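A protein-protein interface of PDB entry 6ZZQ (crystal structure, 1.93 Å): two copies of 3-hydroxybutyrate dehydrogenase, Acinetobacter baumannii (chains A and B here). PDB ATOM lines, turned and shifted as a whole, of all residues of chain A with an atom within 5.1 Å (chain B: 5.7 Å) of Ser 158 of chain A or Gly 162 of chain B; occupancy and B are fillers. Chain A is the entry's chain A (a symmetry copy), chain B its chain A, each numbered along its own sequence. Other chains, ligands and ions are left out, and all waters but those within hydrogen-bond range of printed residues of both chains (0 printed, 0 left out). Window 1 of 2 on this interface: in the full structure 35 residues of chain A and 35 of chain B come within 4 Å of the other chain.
O of Asn 157 of chain A lies within hydrogen-bond range of ND1 of His 161 of chain A (2.9 Å). The backbone carbonyl oxygen of Lys 153 of chain A lies close to the side-chain amide oxygen of Asn 157 of chain A (3.4 Å). A ring nitrogen (ND1) of His 161 of chain B lies within hydrogen-bond range of the backbone carbonyl oxygen (O) of Asn 157 of chain B (2.9 Å). The backbone carbonyl oxygen (O) of Ala 154 of chain A is in hydrogen-bond range of the side-chain hydroxyl (OG) of Ser 158 of chain A (2.5 Å).
Among the printed residues, merely in contact across the chains: His 161 of chain A with His 161 of chain B (3.3 Å), Ser 158 of chain A with Gly 162 of chain B (3.3 Å), Gly 162 of chain A with Ser 158 of chain B (3.3 Å), His 161 of chain A with Gly 165 of chain B (3.3 Å), Ser 158 of chain A with Leu 166 of chain B (3.4 Å), Asn 157 of chain A with Val 169 of chain B (3.4 Å), Ala 154 of chain A with Val 169 of chain B (3.7 Å), Lys 153 of chain A with Val 169 of chain B (3.8 Å), Ser 158 of chain A with Leu 116 of chain B (3.9 Å), Gly 162 of chain A with Gly 162 of chain B (3.9 Å) and Phe 108 of chain A with Leu 116 of chain B (3.9 Å).
Of chain B, only Leu 116 (3.9 Å), Gly 162 (3.3 Å) and Leu 166 (3.4 Å) come within 4 Å of Ser 158 of chain A. Gly 162 of chain B touches two residues of chain A. Of the printed residues of chain A, Val 169 of chain B touches Lys 153, Ala 154 and Asn 157. Printed residues of chain A within 4 Å of Leu 166 of chain B: Ser 158. Of the printed residues of chain B, Gly 162 of chain A touches Ser 158 and Gly 162. Printed residues of chain B within 4 Å of Asn 157 of chain A: Val 169 (3.4 Å). Lys 160 of chain A touches none of the printed residues of chain B. The nearest residue of chain A that does not touch Gly 162 of chain B is His 161 of chain A (4.1 Å). The nearest printed residue of chain A that does not touch His 161 of chain B is Gly 162 of chain A (4.1 Å).
Of the 12 printed residues of chain A, 7 touch a printed residue of chain B. Hydrophobic or aromatic side chains of chain A that line the printed part of chain B: Phe 108 and His 161. Of the 13 printed residues of chain B, 7 touch a printed residue of chain A. Hydrophobic or aromatic side chains of chain B within 4 Å of the printed part of chain A: Leu 116, His 161, Leu 166 and Val 169.
Ser 158 of chain A touches Gly 162 of chain B, and with the chains exchanged Gly 162 of chain A touches Ser 158 of chain B. His 161 of chain B touches its own counterpart, His 161 of chain A. Gly 162 of chain A touches its own counterpart, Gly 162 of chain B. Positions printed for both chains: 157, 158, 159, 160, 161 and 162.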
ATOM      1  N   PHE A 108      28.816  23.906 -25.242  1.00  0.00           N
ATOM      2  CA  PHE A 108      28.094  22.851 -24.494  1.00  0.00           C
ATOM      3  C   PHE A 108      26.705  23.370 -24.067  1.00  0.00           C
ATOM      4  O   PHE A 108      25.678  22.739 -24.396  1.00  0.00           O
ATOM      5  CB  PHE A 108      28.843  22.450 -23.237  1.00  0.00           C
ATOM      6  CG  PHE A 108      28.230  21.272 -22.537  1.00  0.00           C
ATOM      7  CD1 PHE A 108      28.572  19.978 -22.909  1.00  0.00           C
ATOM      8  CD2 PHE A 108      27.356  21.454 -21.477  1.00  0.00           C
ATOM      9  CE1 PHE A 108      28.038  18.893 -22.236  1.00  0.00           C
ATOM     10  CE2 PHE A 108      26.813  20.364 -20.814  1.00  0.00           C
ATOM     11  CZ  PHE A 108      27.158  19.087 -21.188  1.00  0.00           C
ATOM     12  N   VAL A 112      22.714  22.418 -25.486  1.00  0.00           N
ATOM     13  CA  VAL A 112      21.693  21.974 -24.495  1.00  0.00           C
ATOM     14  C   VAL A 112      20.488  22.937 -24.528  1.00  0.00           C
ATOM     15  O   VAL A 112      19.324  22.472 -24.641  1.00  0.00           O
ATOM     16  CB  VAL A 112      22.313  21.845 -23.095  1.00  0.00           C
ATOM     17  CG1 VAL A 112      21.247  21.670 -22.025  1.00  0.00           C
ATOM     18  CG2 VAL A 112      23.325  20.713 -23.036  1.00  0.00           C
ATOM     19  N   LYS A 153      31.218  14.309 -28.866  1.00  0.00           N
ATOM     20  CA  LYS A 153      29.833  14.873 -28.936  1.00  0.00           C
ATOM     21  C   LYS A 153      29.264  15.085 -27.533  1.00  0.00           C
ATOM     22  O   LYS A 153      28.082  14.696 -27.304  1.00  0.00           O
ATOM     23  CB  LYS A 153      28.952  13.954 -29.790  1.00  0.00           C
ATOM     24  CG  LYS A 153      29.272  13.999 -31.272  1.00  0.00           C
ATOM     25  CD  LYS A 153      28.514  13.024 -32.113  1.00  0.00           C
ATOM     26  CE  LYS A 153      28.726  13.276 -33.583  1.00  0.00           C
ATOM     27  NZ  LYS A 153      28.436  12.077 -34.391  1.00  0.00           N
ATOM     28  N   ALA A 154      30.066  15.666 -26.637  1.00  0.00           N
ATOM     29  CA  ALA A 154      29.729  15.876 -25.210  1.00  0.00           C
ATOM     30  C   ALA A 154      28.373  16.597 -25.112  1.00  0.00           C
ATOM     31  O   ALA A 154      27.427  16.063 -24.456  1.00  0.00           O
ATOM     32  CB  ALA A 154      30.826  16.656 -24.549  1.00  0.00           C
ATOM     33  N   GLY A 155      28.274  17.752 -25.772  1.00  0.00           N
ATOM     34  CA  GLY A 155      27.079  18.620 -25.734  1.00  0.00           C
ATOM     35  C   GLY A 155      25.906  17.993 -26.458  1.00  0.00           C
ATOM     36  O   GLY A 155      24.781  17.994 -25.905  1.00  0.00           O
ATOM     37  N   TYR A 156      26.121  17.499 -27.672  1.00  0.00           N
ATOM     38  CA  TYR A 156      25.044  16.891 -28.490  1.00  0.00           C
ATOM     39  C   TYR A 156      24.459  15.690 -27.736  1.00  0.00           C
ATOM     40  O   TYR A 156      23.239  15.619 -27.548  1.00  0.00           O
ATOM     41  CB  TYR A 156      25.575  16.546 -29.878  1.00  0.00           C
ATOM     42  CG  TYR A 156      24.545  16.108 -30.881  1.00  0.00           C
ATOM     43  CD1 TYR A 156      24.161  14.779 -31.004  1.00  0.00           C
ATOM     44  CD2 TYR A 156      23.980  17.024 -31.755  1.00  0.00           C
ATOM     45  CE1 TYR A 156      23.238  14.382 -31.956  1.00  0.00           C
ATOM     46  CE2 TYR A 156      23.047  16.651 -32.696  1.00  0.00           C
ATOM     47  CZ  TYR A 156      22.676  15.324 -32.800  1.00  0.00           C
ATOM     48  OH  TYR A 156      21.743  14.985 -33.734  1.00  0.00           O
ATOM     49  N   ASN A 157      25.298  14.749 -27.323  1.00  0.00           N
ATOM     50  CA  ASN A 157      24.816  13.470 -26.748  1.00  0.00           C
ATOM     51  C   ASN A 157      24.122  13.762 -25.420  1.00  0.00           C
ATOM     52  O   ASN A 157      23.092  13.134 -25.174  1.00  0.00           O
ATOM     53  CB  ASN A 157      25.926  12.427 -26.607  1.00  0.00           C
ATOM     54  CG  ASN A 157      26.214  11.781 -27.941  1.00  0.00           C
ATOM     55  OD1 ASN A 157      26.213  12.466 -28.965  1.00  0.00           O
ATOM     56  ND2 ASN A 157      26.362  10.467 -27.958  1.00  0.00           N
ATOM     57  N   SER A 158      24.656  14.713 -24.644  1.00  0.00           N
ATOM     58  CA  SER A 158      24.091  15.207 -23.365  1.00  0.00           C
ATOM     59  C   SER A 158      22.685  15.785 -23.615  1.00  0.00           C
ATOM     60  O   SER A 158      21.769  15.406 -22.899  1.00  0.00           O
ATOM     61  CB  SER A 158      25.004  16.211 -22.720  1.00  0.00           C
ATOM     62  OG  SER A 158      26.240  15.626 -22.248  1.00  0.00           O
ATOM     63  N   ALA A 159      22.529  16.646 -24.620  1.00  0.00           N
ATOM     64  CA  ALA A 159      21.256  17.301 -24.975  1.00  0.00           C
ATOM     65  C   ALA A 159      20.273  16.241 -25.484  1.00  0.00           C
ATOM     66  O   ALA A 159      19.127  16.234 -24.987  1.00  0.00           O
ATOM     67  CB  ALA A 159      21.480  18.393 -25.972  1.00  0.00           C
ATOM     68  N   LYS A 160      20.696  15.354 -26.391  1.00  0.00           N
ATOM     69  CA  LYS A 160      19.780  14.330 -26.957  1.00  0.00           C
ATOM     70  C   LYS A 160      19.336  13.325 -25.882  1.00  0.00           C
ATOM     71  O   LYS A 160      18.144  12.927 -25.905  1.00  0.00           O
ATOM     72  CB  LYS A 160      20.395  13.624 -28.164  1.00  0.00           C
ATOM     73  CG  LYS A 160      20.547  14.462 -29.429  1.00  0.00           C
ATOM     74  CD  LYS A 160      19.394  15.387 -29.781  1.00  0.00           C
ATOM     75  CE  LYS A 160      19.448  15.768 -31.254  1.00  0.00           C
ATOM     76  NZ  LYS A 160      18.284  16.561 -31.714  1.00  0.00           N
ATOM     77  N   HIS A 161      20.243  12.897 -25.002  1.00  0.00           N
ATOM     78  CA  HIS A 161      19.929  12.039 -23.828  1.00  0.00           C
ATOM     79  C   HIS A 161      18.882  12.759 -22.974  1.00  0.00           C
ATOM     80  O   HIS A 161      17.904  12.130 -22.599  1.00  0.00           O
ATOM     81  CB  HIS A 161      21.175  11.693 -23.009  1.00  0.00           C
ATOM     82  CG  HIS A 161      21.844  10.424 -23.431  1.00  0.00           C
ATOM     83  ND1 HIS A 161      22.491  10.293 -24.662  1.00  0.00           N
ATOM     84  CD2 HIS A 161      21.913   9.214 -22.827  1.00  0.00           C
ATOM     85  CE1 HIS A 161      22.964   9.055 -24.753  1.00  0.00           C
ATOM     86  NE2 HIS A 161      22.615   8.377 -23.647  1.00  0.00           N
ATOM     87  N   GLY A 162      19.092  14.052 -22.740  1.00  0.00           N
ATOM     88  CA  GLY A 162      18.204  14.907 -21.939  1.00  0.00           C
ATOM     89  C   GLY A 162      16.795  14.975 -22.513  1.00  0.00           C
ATOM     90  O   GLY A 162      15.852  14.855 -21.732  1.00  0.00           O
ATOM     91  N   LEU B 116      24.081  18.760 -14.879  1.00  0.00           N
ATOM     92  CA  LEU B 116      24.701  18.341 -16.151  1.00  0.00           C
ATOM     93  C   LEU B 116      25.932  19.215 -16.396  1.00  0.00           C
ATOM     94  O   LEU B 116      27.048  18.665 -16.415  1.00  0.00           O
ATOM     95  CB  LEU B 116      23.676  18.439 -17.282  1.00  0.00           C
ATOM     96  CG  LEU B 116      24.198  18.181 -18.690  1.00  0.00           C
ATOM     97  CD1 LEU B 116      24.978  16.874 -18.768  1.00  0.00           C
ATOM     98  CD2 LEU B 116      23.068  18.173 -19.702  1.00  0.00           C
ATOM     99  N   ASN B 157      14.806  15.018 -14.378  1.00  0.00           N
ATOM    100  CA  ASN B 157      14.917  13.789 -15.202  1.00  0.00           C
ATOM    101  C   ASN B 157      15.704  14.119 -16.468  1.00  0.00           C
ATOM    102  O   ASN B 157      16.516  13.282 -16.860  1.00  0.00           O
ATOM    103  CB  ASN B 157      13.559  13.157 -15.510  1.00  0.00           C
ATOM    104  CG  ASN B 157      13.060  12.377 -14.318  1.00  0.00           C
ATOM    105  OD1 ASN B 157      13.228  12.822 -13.181  1.00  0.00           O
ATOM    106  ND2 ASN B 157      12.540  11.183 -14.549  1.00  0.00           N
ATOM    107  N   SER B 158      15.488  15.315 -17.031  1.00  0.00           N
ATOM    108  CA  SER B 158      16.206  15.862 -18.207  1.00  0.00           C
ATOM    109  C   SER B 158      17.712  15.953 -17.891  1.00  0.00           C
ATOM    110  O   SER B 158      18.500  15.472 -18.692  1.00  0.00           O
ATOM    111  CB  SER B 158      15.640  17.191 -18.621  1.00  0.00           C
ATOM    112  OG  SER B 158      14.302  17.088 -19.160  1.00  0.00           O
ATOM    113  N   ALA B 159      18.080  16.523 -16.744  1.00  0.00           N
ATOM    114  CA  ALA B 159      19.477  16.703 -16.306  1.00  0.00           C
ATOM    115  C   ALA B 159      20.099  15.328 -16.038  1.00  0.00           C
ATOM    116  O   ALA B 159      21.208  15.089 -16.560  1.00  0.00           O
ATOM    117  CB  ALA B 159      19.547  17.600 -15.111  1.00  0.00           C
ATOM    118  N   LYS B 160      19.413  14.443 -15.308  1.00  0.00           N
ATOM    119  CA  LYS B 160      19.980  13.110 -14.975  1.00  0.00           C
ATOM    120  C   LYS B 160      20.147  12.247 -16.236  1.00  0.00           C
ATOM    121  O   LYS B 160      21.173  11.527 -16.325  1.00  0.00           O
ATOM    122  CB  LYS B 160      19.154  12.392 -13.910  1.00  0.00           C
ATOM    123  CG  LYS B 160      19.213  12.978 -12.504  1.00  0.00           C
ATOM    124  CD  LYS B 160      20.573  13.447 -12.013  1.00  0.00           C
ATOM    125  CE  LYS B 160      20.589  13.537 -10.494  1.00  0.00           C
ATOM    126  NZ  LYS B 160      21.917  13.858  -9.923  1.00  0.00           N
ATOM    127  N   HIS B 161      19.181  12.275 -17.156  1.00  0.00           N
ATOM    128  CA  HIS B 161      19.269  11.605 -18.481  1.00  0.00           C
ATOM    129  C   HIS B 161      20.502  12.145 -19.210  1.00  0.00           C
ATOM    130  O   HIS B 161      21.269  11.346 -19.727  1.00  0.00           O
ATOM    131  CB  HIS B 161      18.000  11.797 -19.316  1.00  0.00           C
ATOM    132  CG  HIS B 161      16.983  10.717 -19.127  1.00  0.00           C
ATOM    133  ND1 HIS B 161      16.291  10.543 -17.927  1.00  0.00           N
ATOM    134  CD2 HIS B 161      16.587   9.717 -19.951  1.00  0.00           C
ATOM    135  CE1 HIS B 161      15.480   9.499 -18.062  1.00  0.00           C
ATOM    136  NE2 HIS B 161      15.650   8.976 -19.288  1.00  0.00           N
ATOM    137  N   GLY B 162      20.679  13.463 -19.185  1.00  0.00           N
ATOM    138  CA  GLY B 162      21.798  14.165 -19.832  1.00  0.00           C
ATOM    139  C   GLY B 162      23.150  13.714 -19.296  1.00  0.00           C
ATOM    140  O   GLY B 162      24.041  13.481 -20.112  1.00  0.00           O
ATOM    141  N   VAL B 163      23.298  13.593 -17.981  1.00  0.00           N
ATOM    142  CA  VAL B 163      24.594  13.231 -17.337  1.00  0.00           C
ATOM    143  C   VAL B 163      24.931  11.763 -17.667  1.00  0.00           C
ATOM    144  O   VAL B 163      26.118  11.407 -17.654  1.00  0.00           O
ATOM    145  CB  VAL B 163      24.611  13.531 -15.818  1.00  0.00           C
ATOM    146  CG1 VAL B 163      24.142  12.379 -14.960  1.00  0.00           C
ATOM    147  CG2 VAL B 163      26.006  13.953 -15.354  1.00  0.00           C
ATOM    148  N   ILE B 164      23.954  10.933 -18.014  1.00  0.00           N
ATOM    149  CA  ILE B 164      24.273   9.541 -18.432  1.00  0.00           C
ATOM    150  C   ILE B 164      24.864   9.607 -19.848  1.00  0.00           C
ATOM    151  O   ILE B 164      25.840   8.882 -20.132  1.00  0.00           O
ATOM    152  CB  ILE B 164      23.029   8.643 -18.317  1.00  0.00           C
ATOM    153  CG1 ILE B 164      22.670   8.413 -16.839  1.00  0.00           C
ATOM    154  CG2 ILE B 164      23.252   7.339 -19.087  1.00  0.00           C
ATOM    155  CD1 ILE B 164      21.407   7.593 -16.601  1.00  0.00           C
ATOM    156  N   GLY B 165      24.306  10.459 -20.702  1.00  0.00           N
ATOM    157  CA  GLY B 165      24.863  10.718 -22.033  1.00  0.00           C
ATOM    158  C   GLY B 165      26.286  11.239 -21.936  1.00  0.00           C
ATOM    159  O   GLY B 165      27.134  10.770 -22.692  1.00  0.00           O
ATOM    160  N   LEU B 166      26.546  12.185 -21.033  1.00  0.00           N
ATOM    161  CA  LEU B 166      27.899  12.778 -20.854  1.00  0.00           C
ATOM    162  C   LEU B 166      28.862  11.689 -20.390  1.00  0.00           C
ATOM    163  O   LEU B 166      30.000  11.650 -20.857  1.00  0.00           O
ATOM    164  CB  LEU B 166      27.819  13.895 -19.815  1.00  0.00           C
ATOM    165  CG  LEU B 166      29.150  14.497 -19.385  1.00  0.00           C
ATOM    166  CD1 LEU B 166      29.847  15.134 -20.565  1.00  0.00           C
ATOM    167  CD2 LEU B 166      28.935  15.506 -18.277  1.00  0.00           C
ATOM    168  N   THR B 167      28.416  10.868 -19.453  1.00  0.00           N
ATOM    169  CA  THR B 167      29.137   9.682 -18.952  1.00  0.00           C
ATOM    170  C   THR B 167      29.619   8.813 -20.116  1.00  0.00           C
ATOM    171  O   THR B 167      30.801   8.440 -20.106  1.00  0.00           O
ATOM    172  CB  THR B 167      28.252   8.892 -17.985  1.00  0.00           C
ATOM    173  OG1 THR B 167      27.933   9.807 -16.946  1.00  0.00           O
ATOM    174  CG2 THR B 167      28.929   7.662 -17.431  1.00  0.00           C
ATOM    175  N   VAL B 169      29.966   9.464 -23.380  1.00  0.00           N
ATOM    176  CA  VAL B 169      30.855  10.242 -24.286  1.00  0.00           C
ATOM    177  C   VAL B 169      32.245  10.334 -23.648  1.00  0.00           C
ATOM    178  O   VAL B 169      33.221  10.007 -24.315  1.00  0.00           O
ATOM    179  CB  VAL B 169      30.278  11.632 -24.579  1.00  0.00           C
ATOM    180  CG1 VAL B 169      31.314  12.498 -25.289  1.00  0.00           C
ATOM    181  CG2 VAL B 169      29.023  11.527 -25.413  1.00  0.00           C
